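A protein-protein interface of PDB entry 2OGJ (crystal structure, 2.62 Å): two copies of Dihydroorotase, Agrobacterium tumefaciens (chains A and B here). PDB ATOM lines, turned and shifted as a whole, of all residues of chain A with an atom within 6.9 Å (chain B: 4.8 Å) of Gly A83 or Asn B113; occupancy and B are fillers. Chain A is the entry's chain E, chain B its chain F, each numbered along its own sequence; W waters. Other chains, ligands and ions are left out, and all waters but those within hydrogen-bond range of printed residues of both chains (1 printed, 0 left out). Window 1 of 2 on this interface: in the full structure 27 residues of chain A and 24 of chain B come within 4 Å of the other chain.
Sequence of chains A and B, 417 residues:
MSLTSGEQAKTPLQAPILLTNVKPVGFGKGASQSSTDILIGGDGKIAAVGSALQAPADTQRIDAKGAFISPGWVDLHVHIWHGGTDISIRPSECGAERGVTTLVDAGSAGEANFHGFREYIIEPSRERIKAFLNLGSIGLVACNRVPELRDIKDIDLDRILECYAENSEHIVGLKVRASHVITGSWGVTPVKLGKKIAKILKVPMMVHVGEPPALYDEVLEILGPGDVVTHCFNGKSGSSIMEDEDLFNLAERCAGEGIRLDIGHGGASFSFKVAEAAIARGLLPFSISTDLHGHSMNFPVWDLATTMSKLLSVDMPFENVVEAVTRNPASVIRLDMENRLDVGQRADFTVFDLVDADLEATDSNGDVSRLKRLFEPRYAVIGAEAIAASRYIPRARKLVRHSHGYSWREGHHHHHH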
ATOM      1  N   ILE A  80      27.111   9.290  19.570  1.00  0.00           N
ATOM      2  CA  ILE A  80      25.760   9.401  19.048  1.00  0.00           C
ATOM      3  C   ILE A  80      24.790  10.152  19.952  1.00  0.00           C
ATOM      4  O   ILE A  80      23.587   9.875  19.942  1.00  0.00           O
ATOM      5  CB  ILE A  80      25.194   8.005  18.776  1.00  0.00           C
ATOM      6  CG1 ILE A  80      25.114   7.204  20.081  1.00  0.00           C
ATOM      7  CG2 ILE A  80      26.098   7.280  17.802  1.00  0.00           C
ATOM      8  CD1 ILE A  80      24.455   5.834  19.943  1.00  0.00           C
ATOM      9  N   TRP A  81      25.302  11.097  20.732  1.00  0.00           N
ATOM     10  CA  TRP A  81      24.437  11.891  21.615  1.00  0.00           C
ATOM     11  C   TRP A  81      23.974  13.083  20.777  1.00  0.00           C
ATOM     12  O   TRP A  81      24.206  14.250  21.116  1.00  0.00           O
ATOM     13  CB  TRP A  81      25.243  12.342  22.842  1.00  0.00           C
ATOM     14  CG  TRP A  81      24.492  13.038  23.973  1.00  0.00           C
ATOM     15  CD1 TRP A  81      25.030  13.416  25.163  1.00  0.00           C
ATOM     16  CD2 TRP A  81      23.110  13.468  24.010  1.00  0.00           C
ATOM     17  NE1 TRP A  81      24.092  14.050  25.934  1.00  0.00           N
ATOM     18  CE2 TRP A  81      22.906  14.097  25.258  1.00  0.00           C
ATOM     19  CE3 TRP A  81      22.034  13.387  23.117  1.00  0.00           C
ATOM     20  CZ2 TRP A  81      21.666  14.643  25.639  1.00  0.00           C
ATOM     21  CZ3 TRP A  81      20.792  13.937  23.499  1.00  0.00           C
ATOM     22  CH2 TRP A  81      20.622  14.554  24.745  1.00  0.00           C
ATOM     23  N   HIS A  82      23.335  12.762  19.656  1.00  0.00           N
ATOM     24  CA  HIS A  82      22.832  13.758  18.710  1.00  0.00           C
ATOM     25  C   HIS A  82      21.965  14.792  19.413  1.00  0.00           C
ATOM     26  O   HIS A  82      21.106  14.434  20.222  1.00  0.00           O
ATOM     27  CB  HIS A  82      22.018  13.069  17.598  1.00  0.00           C
ATOM     28  CG  HIS A  82      21.432  14.022  16.604  1.00  0.00           C
ATOM     29  ND1 HIS A  82      22.182  14.616  15.608  1.00  0.00           N
ATOM     30  CD2 HIS A  82      20.185  14.539  16.499  1.00  0.00           C
ATOM     31  CE1 HIS A  82      21.420  15.463  14.937  1.00  0.00           C
ATOM     32  NE2 HIS A  82      20.206  15.436  15.457  1.00  0.00           N
ATOM     33  N   GLY A  83      22.187  16.070  19.102  1.00  0.00           N
ATOM     34  CA  GLY A  83      21.407  17.122  19.738  1.00  0.00           C
ATOM     35  C   GLY A  83      21.979  17.672  21.047  1.00  0.00           C
ATOM     36  O   GLY A  83      22.141  18.882  21.198  1.00  0.00           O
ATOM     37  N   GLY A  84      22.285  16.787  21.995  1.00  0.00           N
ATOM     38  CA  GLY A  84      22.822  17.209  23.278  1.00  0.00           C
ATOM     39  C   GLY A  84      24.238  17.752  23.196  1.00  0.00           C
ATOM     40  O   GLY A  84      24.566  18.767  23.811  1.00  0.00           O
ATOM     41  N   THR A  85      25.092  17.054  22.462  1.00  0.00           N
ATOM     42  CA  THR A  85      26.464  17.495  22.279  1.00  0.00           C
ATOM     43  C   THR A  85      26.479  18.201  20.931  1.00  0.00           C
ATOM     44  O   THR A  85      25.416  18.474  20.364  1.00  0.00           O
ATOM     45  CB  THR A  85      27.434  16.310  22.236  1.00  0.00           C
ATOM     46  OG1 THR A  85      27.203  15.546  21.044  1.00  0.00           O
ATOM     47  CG2 THR A  85      27.237  15.433  23.454  1.00  0.00           C
ATOM     48  N   ASP A  86      27.665  18.475  20.399  1.00  0.00           N
ATOM     49  CA  ASP A  86      27.767  19.172  19.118  1.00  0.00           C
ATOM     50  C   ASP A  86      28.492  18.320  18.083  1.00  0.00           C
ATOM     51  O   ASP A  86      28.368  18.527  16.879  1.00  0.00           O
ATOM     52  CB  ASP A  86      28.529  20.503  19.310  1.00  0.00           C
ATOM     53  CG  ASP A  86      30.025  20.298  19.603  1.00  0.00           C
ATOM     54  OD1 ASP A  86      30.380  19.228  20.140  1.00  0.00           O
ATOM     55  OD2 ASP A  86      30.854  21.200  19.318  1.00  0.00           O
ATOM     56  N   SER A  88      28.331  14.771  18.027  1.00  0.00           N
ATOM     57  CA  SER A  88      27.617  13.509  17.793  1.00  0.00           C
ATOM     58  C   SER A  88      26.860  13.366  16.482  1.00  0.00           C
ATOM     59  O   SER A  88      26.285  14.332  15.962  1.00  0.00           O
ATOM     60  CB  SER A  88      26.602  13.269  18.915  1.00  0.00           C
ATOM     61  OG  SER A  88      27.216  12.974  20.147  1.00  0.00           O
ATOM     62  N   ILE A  89      26.836  12.146  15.959  1.00  0.00           N
ATOM     63  CA  ILE A  89      26.068  11.891  14.746  1.00  0.00           C
ATOM     64  C   ILE A  89      24.822  11.130  15.201  1.00  0.00           C
ATOM     65  O   ILE A  89      24.647  10.883  16.399  1.00  0.00           O
ATOM     66  CB  ILE A  89      26.847  11.056  13.716  1.00  0.00           C
ATOM     67  CG1 ILE A  89      27.234   9.715  14.323  1.00  0.00           C
ATOM     68  CG2 ILE A  89      28.083  11.821  13.242  1.00  0.00           C
ATOM     69  CD1 ILE A  89      28.204   8.935  13.483  1.00  0.00           C
ATOM     70  N   ASN A 113      23.971  15.376  31.789  1.00  0.00           N
ATOM     71  CA  ASN A 113      22.831  15.148  30.910  1.00  0.00           C
ATOM     72  C   ASN A 113      22.725  13.741  30.349  1.00  0.00           C
ATOM     73  O   ASN A 113      22.319  13.574  29.186  1.00  0.00           O
ATOM     74  CB  ASN A 113      22.793  16.155  29.736  1.00  0.00           C
ATOM     75  CG  ASN A 113      23.906  15.936  28.713  1.00  0.00           C
ATOM     76  OD1 ASN A 113      24.536  14.872  28.653  1.00  0.00           O
ATOM     77  ND2 ASN A 113      24.146  16.954  27.893  1.00  0.00           N
ATOM     78  N   ILE A 121      18.221   9.047  22.784  1.00  0.00           N
ATOM     79  CA  ILE A 121      19.021   8.133  21.989  1.00  0.00           C
ATOM     80  C   ILE A 121      18.838   6.655  22.250  1.00  0.00           C
ATOM     81  O   ILE A 121      18.613   5.887  21.316  1.00  0.00           O
ATOM     82  CB  ILE A 121      20.536   8.449  22.138  1.00  0.00           C
ATOM     83  CG1 ILE A 121      20.789   9.923  21.835  1.00  0.00           C
ATOM     84  CG2 ILE A 121      21.358   7.556  21.214  1.00  0.00           C
ATOM     85  CD1 ILE A 121      20.258  10.392  20.477  1.00  0.00           C
ATOM     86  N   VAL A 141      29.708  18.288  25.037  1.00  0.00           N
ATOM     87  CA  VAL A 141      28.797  19.302  24.491  1.00  0.00           C
ATOM     88  C   VAL A 141      29.461  20.207  23.445  1.00  0.00           C
ATOM     89  O   VAL A 141      28.875  20.522  22.413  1.00  0.00           O
ATOM     90  CB  VAL A 141      28.256  20.258  25.584  1.00  0.00           C
ATOM     91  CG1 VAL A 141      26.744  20.142  25.691  1.00  0.00           C
ATOM     92  CG2 VAL A 141      28.952  19.993  26.903  1.00  0.00           C
ATOM     93  N   ALA A 142      30.673  20.648  23.756  1.00  0.00           N
ATOM     94  CA  ALA A 142      31.449  21.516  22.893  1.00  0.00           C
ATOM     95  C   ALA A 142      32.817  20.851  22.801  1.00  0.00           C
ATOM     96  O   ALA A 142      33.859  21.428  23.138  1.00  0.00           O
ATOM     97  CB  ALA A 142      31.552  22.893  23.524  1.00  0.00           C
ATOM     98  N   ARG A 145      36.424  22.240  22.590  1.00  0.00           N
ATOM     99  CA  ARG A 145      36.452  23.691  22.644  1.00  0.00           C
ATOM    100  C   ARG A 145      36.265  24.151  24.078  1.00  0.00           C
ATOM    101  O   ARG A 145      36.741  25.213  24.467  1.00  0.00           O
ATOM    102  CB  ARG A 145      35.381  24.273  21.717  1.00  0.00           C
ATOM    103  CG  ARG A 145      35.636  23.912  20.254  1.00  0.00           C
ATOM    104  CD  ARG A 145      34.600  24.495  19.333  1.00  0.00           C
ATOM    105  NE  ARG A 145      33.298  23.872  19.507  1.00  0.00           N
ATOM    106  CZ  ARG A 145      32.226  24.524  19.920  1.00  0.00           C
ATOM    107  NH1 ARG A 145      32.321  25.814  20.201  1.00  0.00           N
ATOM    108  NH2 ARG A 145      31.070  23.891  20.039  1.00  0.00           N
ATOM    109  N   TRP B  81      15.129  23.045  28.196  1.00  0.00           N
ATOM    110  CA  TRP B  81      16.002  22.268  27.310  1.00  0.00           C
ATOM    111  C   TRP B  81      16.145  20.914  28.000  1.00  0.00           C
ATOM    112  O   TRP B  81      17.244  20.469  28.340  1.00  0.00           O
ATOM    113  CB  TRP B  81      17.357  22.960  27.166  1.00  0.00           C
ATOM    114  CG  TRP B  81      18.313  22.398  26.125  1.00  0.00           C
ATOM    115  CD1 TRP B  81      19.492  22.958  25.741  1.00  0.00           C
ATOM    116  CD2 TRP B  81      18.221  21.145  25.417  1.00  0.00           C
ATOM    117  NE1 TRP B  81      20.150  22.139  24.851  1.00  0.00           N
ATOM    118  CE2 TRP B  81      19.393  21.022  24.634  1.00  0.00           C
ATOM    119  CE3 TRP B  81      17.266  20.118  25.367  1.00  0.00           C
ATOM    120  CZ2 TRP B  81      19.635  19.912  23.811  1.00  0.00           C
ATOM    121  CZ3 TRP B  81      17.507  19.014  24.548  1.00  0.00           C
ATOM    122  CH2 TRP B  81      18.680  18.923  23.784  1.00  0.00           C
ATOM    123  N   GLY B  84      18.866  17.628  27.472  1.00  0.00           N
ATOM    124  CA  GLY B  84      20.161  18.155  27.070  1.00  0.00           C
ATOM    125  C   GLY B  84      20.782  18.993  28.170  1.00  0.00           C
ATOM    126  O   GLY B  84      21.964  19.346  28.137  1.00  0.00           O
ATOM    127  N   ALA B 109      20.565  26.845  26.284  1.00  0.00           N
ATOM    128  CA  ALA B 109      21.436  26.383  25.215  1.00  0.00           C
ATOM    129  C   ALA B 109      22.344  27.476  24.682  1.00  0.00           C
ATOM    130  O   ALA B 109      21.958  28.652  24.658  1.00  0.00           O
ATOM    131  CB  ALA B 109      20.601  25.810  24.066  1.00  0.00           C
ATOM    132  N   GLY B 110      23.546  27.052  24.282  1.00  0.00           N
ATOM    133  CA  GLY B 110      24.535  27.929  23.696  1.00  0.00           C
ATOM    134  C   GLY B 110      24.691  27.501  22.251  1.00  0.00           C
ATOM    135  O   GLY B 110      23.896  26.714  21.762  1.00  0.00           O
ATOM    136  N   GLU B 111      25.707  27.996  21.559  1.00  0.00           N
ATOM    137  CA  GLU B 111      25.894  27.629  20.162  1.00  0.00           C
ATOM    138  C   GLU B 111      26.181  26.141  19.979  1.00  0.00           C
ATOM    139  O   GLU B 111      25.796  25.538  18.977  1.00  0.00           O
ATOM    140  CB  GLU B 111      27.015  28.478  19.536  1.00  0.00           C
ATOM    141  CG  GLU B 111      28.371  28.438  20.243  1.00  0.00           C
ATOM    142  CD  GLU B 111      29.143  27.142  20.016  1.00  0.00           C
ATOM    143  OE1 GLU B 111      28.749  26.376  19.116  1.00  0.00           O
ATOM    144  OE2 GLU B 111      30.153  26.894  20.728  1.00  0.00           O
ATOM    145  N   ALA B 112      26.843  25.550  20.961  1.00  0.00           N
ATOM    146  CA  ALA B 112      27.203  24.138  20.916  1.00  0.00           C
ATOM    147  C   ALA B 112      26.055  23.152  20.661  1.00  0.00           C
ATOM    148  O   ALA B 112      26.139  22.356  19.732  1.00  0.00           O
ATOM    149  CB  ALA B 112      27.927  23.764  22.183  1.00  0.00           C
ATOM    150  N   ASN B 113      24.991  23.195  21.466  1.00  0.00           N
ATOM    151  CA  ASN B 113      23.882  22.260  21.273  1.00  0.00           C
ATOM    152  C   ASN B 113      22.513  22.842  21.038  1.00  0.00           C
ATOM    153  O   ASN B 113      21.526  22.244  21.462  1.00  0.00           O
ATOM    154  CB  ASN B 113      23.759  21.293  22.450  1.00  0.00           C
ATOM    155  CG  ASN B 113      23.353  21.980  23.746  1.00  0.00           C
ATOM    156  OD1 ASN B 113      22.846  23.104  23.755  1.00  0.00           O
ATOM    157  ND2 ASN B 113      23.558  21.287  24.853  1.00  0.00           N
ATOM    158  N   PHE B 114      22.422  23.988  20.371  1.00  0.00           N
ATOM    159  CA  PHE B 114      21.105  24.571  20.103  1.00  0.00           C
ATOM    160  C   PHE B 114      20.255  23.709  19.143  1.00  0.00           C
ATOM    161  O   PHE B 114      19.031  23.623  19.294  1.00  0.00           O
ATOM    162  CB  PHE B 114      21.232  25.986  19.521  1.00  0.00           C
ATOM    163  CG  PHE B 114      19.903  26.648  19.274  1.00  0.00           C
ATOM    164  CD1 PHE B 114      19.242  27.304  20.299  1.00  0.00           C
ATOM    165  CD2 PHE B 114      19.267  26.524  18.041  1.00  0.00           C
ATOM    166  CE1 PHE B 114      17.967  27.814  20.108  1.00  0.00           C
ATOM    167  CE2 PHE B 114      17.984  27.038  17.843  1.00  0.00           C
ATOM    168  CZ  PHE B 114      17.335  27.679  18.879  1.00  0.00           C
ATOM    169  N   HIS B 115      20.897  23.076  18.161  1.00  0.00           N
ATOM    170  CA  HIS B 115      20.160  22.262  17.200  1.00  0.00           C
ATOM    171  C   HIS B 115      19.356  21.221  17.924  1.00  0.00           C
ATOM    172  O   HIS B 115      18.231  20.914  17.528  1.00  0.00           O
ATOM    173  CB  HIS B 115      21.090  21.588  16.180  1.00  0.00           C
ATOM    174  CG  HIS B 115      22.104  20.656  16.774  1.00  0.00           C
ATOM    175  ND1 HIS B 115      23.088  21.083  17.639  1.00  0.00           N
ATOM    176  CD2 HIS B 115      22.366  19.354  16.522  1.00  0.00           C
ATOM    177  CE1 HIS B 115      23.919  20.088  17.885  1.00  0.00           C
ATOM    178  NE2 HIS B 115      23.506  19.028  17.218  1.00  0.00           N
ATOM    179  N   GLY B 116      19.941  20.699  18.998  1.00  0.00           N
ATOM    180  CA  GLY B 116      19.279  19.694  19.807  1.00  0.00           C
ATOM    181  C   GLY B 116      18.031  20.244  20.455  1.00  0.00           C
ATOM    182  O   GLY B 116      17.037  19.532  20.579  1.00  0.00           O
ATOM    183  N   PHE B 117      18.085  21.504  20.874  1.00  0.00           N
ATOM    184  CA  PHE B 117      16.939  22.164  21.496  1.00  0.00           C
ATOM    185  C   PHE B 117      15.862  22.325  20.435  1.00  0.00           C
ATOM    186  O   PHE B 117      14.675  22.128  20.701  1.00  0.00           O
ATOM    187  CB  PHE B 117      17.340  23.553  22.022  1.00  0.00           C
ATOM    188  CG  PHE B 117      16.211  24.319  22.660  1.00  0.00           C
ATOM    189  CD1 PHE B 117      15.687  23.924  23.881  1.00  0.00           C
ATOM    190  CD2 PHE B 117      15.652  25.422  22.026  1.00  0.00           C
ATOM    191  CE1 PHE B 117      14.627  24.609  24.456  1.00  0.00           C
ATOM    192  CE2 PHE B 117      14.577  26.114  22.610  1.00  0.00           C
ATOM    193  CZ  PHE B 117      14.073  25.703  23.818  1.00  0.00           C
ATOM    194  N   TYR B 120      14.487  18.503  19.544  1.00  0.00           N
ATOM    195  CA  TYR B 120      13.749  17.863  20.631  1.00  0.00           C
ATOM    196  C   TYR B 120      12.729  18.719  21.357  1.00  0.00           C
ATOM    197  O   TYR B 120      11.766  18.184  21.887  1.00  0.00           O
ATOM    198  CB  TYR B 120      14.719  17.301  21.672  1.00  0.00           C
ATOM    199  CG  TYR B 120      15.756  16.352  21.126  1.00  0.00           C
ATOM    200  CD1 TYR B 120      15.390  15.274  20.327  1.00  0.00           C
ATOM    201  CD2 TYR B 120      17.103  16.509  21.442  1.00  0.00           C
ATOM    202  CE1 TYR B 120      16.336  14.372  19.858  1.00  0.00           C
ATOM    203  CE2 TYR B 120      18.062  15.612  20.979  1.00  0.00           C
ATOM    204  CZ  TYR B 120      17.663  14.541  20.187  1.00  0.00           C
ATOM    205  OH  TYR B 120      18.566  13.607  19.734  1.00  0.00           O
ATOM    206  N   SER B 137      28.992  28.833  25.162  1.00  0.00           N
ATOM    207  CA  SER B 137      28.724  27.631  24.367  1.00  0.00           C
ATOM    208  C   SER B 137      27.996  26.443  25.015  1.00  0.00           C
ATOM    209  O   SER B 137      27.028  25.931  24.442  1.00  0.00           O
ATOM    210  CB  SER B 137      30.029  27.130  23.753  1.00  0.00           C
ATOM    211  OG  SER B 137      30.551  28.123  22.900  1.00  0.00           O
ATOM    212  N   ILE B 138      28.455  25.992  26.183  1.00  0.00           N
ATOM    213  CA  ILE B 138      27.841  24.841  26.833  1.00  0.00           C
ATOM    214  C   ILE B 138      26.476  25.142  27.438  1.00  0.00           C
ATOM    215  O   ILE B 138      25.761  24.239  27.863  1.00  0.00           O
ATOM    216  CB  ILE B 138      28.759  24.256  27.924  1.00  0.00           C
ATOM    217  CG1 ILE B 138      28.903  25.242  29.090  1.00  0.00           C
ATOM    218  CG2 ILE B 138      30.123  23.942  27.327  1.00  0.00           C
ATOM    219  CD1 ILE B 138      29.868  24.770  30.193  1.00  0.00           C
HETATM  220  O   HOH W   1      24.687  16.316  17.530  1.00  0.00           O
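The side-chain hydroxyl of Tyr B120 sits at hydrogen-bond distance from the backbone carbonyl oxygen of His A82, at 2.7 Å.
The backbone carbonyl oxygen of Gly A84 sits at hydrogen-bond distance from the side-chain amide nitrogen of Asn B113 (2.9 Å).
The backbone carbonyl oxygen (O) of Gly B84 sits at hydrogen-bond distance from the side-chain amide nitrogen (ND2) of Asn A113.
The side-chain carboxylate (OE2) of Glu B111 is in salt-bridge range of the guanidinium group (NH1) of Arg A145, 2.5 Å away.
O of Asn B113 sits close to O of Gly A83, 3.4 Å away.
The backbone carbonyl oxygen (O) of Trp A81 lies within hydrogen-bond range of the side-chain hydroxyl (OG1) of Thr A85 (3.3 Å).
The indole nitrogen (NE1) of Trp A81 lies within hydrogen-bond range of the side-chain amide oxygen (OD1) of Asn A113.
OG1 of Thr A85 is in hydrogen-bond range of OG of Ser A88 (2.7 Å).
The side-chain carboxylate (OD2) of Asp A86 lies within salt-bridge range of the guanidinium group (NH2) of Arg A145, at 2.8 Å.
NE1 of Trp B81 lies within hydrogen-bond range of OD1 of Asn B113 (3.1 Å).
OG of Ser B137 lies within hydrogen-bond range of OE2 of Glu B111 (2.5 Å).
CE2 of Tyr B120 touches CA of Gly A83, at 3.9 Å.
Ala B112 touches Thr A85.
Thr A85 touches Asn B113.
His B115 touches Thr A85 (CE1 to O, 3.3 Å).
Asp A86 touches Ala B112.
Val A141 touches Ala B112 (O to CB, 3.4 Å).
Asn B113 touches Val A141 (ND2 to CG1, 3.5 Å).
Ala B112 touches Ala A142.
Arg A145 touches Ala B112.
OG of Ser B137 touches NH1 of Arg A145 (3.97 Å).
Asn B113 touches just these residues of chain A: Gly A83 (3.2 Å), Gly A84 (2.9 Å), Thr A85 (3.9 Å) and Val A141 (3.5 Å).
Of the printed residues of chain A, Trp B81 touches Gly A83.
Printed residues of chain A within 4 Å of Ala B112: Thr A85 (3.999 Å), Asp A86 (3.1 Å), Val A141 (3.4 Å), Ala A142 (3.96 Å) and Arg A145 (3.8 Å).
Ser A88 touches none of the printed residues of chain B.
Gly B110 touches none of the printed residues of chain A.
The nearest printed residue of chain B that does not touch Gly A83 is Phe B117 (4.8 Å).
The nearest printed residue of chain A that does not touch Gly B84 is Trp A81 (4.1 Å).
Printed residues of chain B that touch a printed residue of chain A: Trp B81, Gly B84, Glu B111, Ala B112, Asn B113, His B115, Gly B116, Tyr B120 and Ser B137.
Hydrophobic or aromatic side chains of chain B that line the printed part of chain A: Trp B81, Ala B112, His B115 and Tyr B120.
Of the 14 printed residues of chain A, 10 touch a printed residue of chain B.
Among the printed residues, Asp or Glu carboxylates within 4 Å of a Lys or Arg side-chain nitrogen of the other chain: Arg A145 with Glu B111.
Gly A84 touches Asn B113, and with the chains exchanged Asn A113 touches Gly B84.
Water W1 lies within hydrogen-bond range of N of Gly A83 (3.0 Å), NE2 of His B115 (3.0 Å) and O of Ser A88 (3.0 Å).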
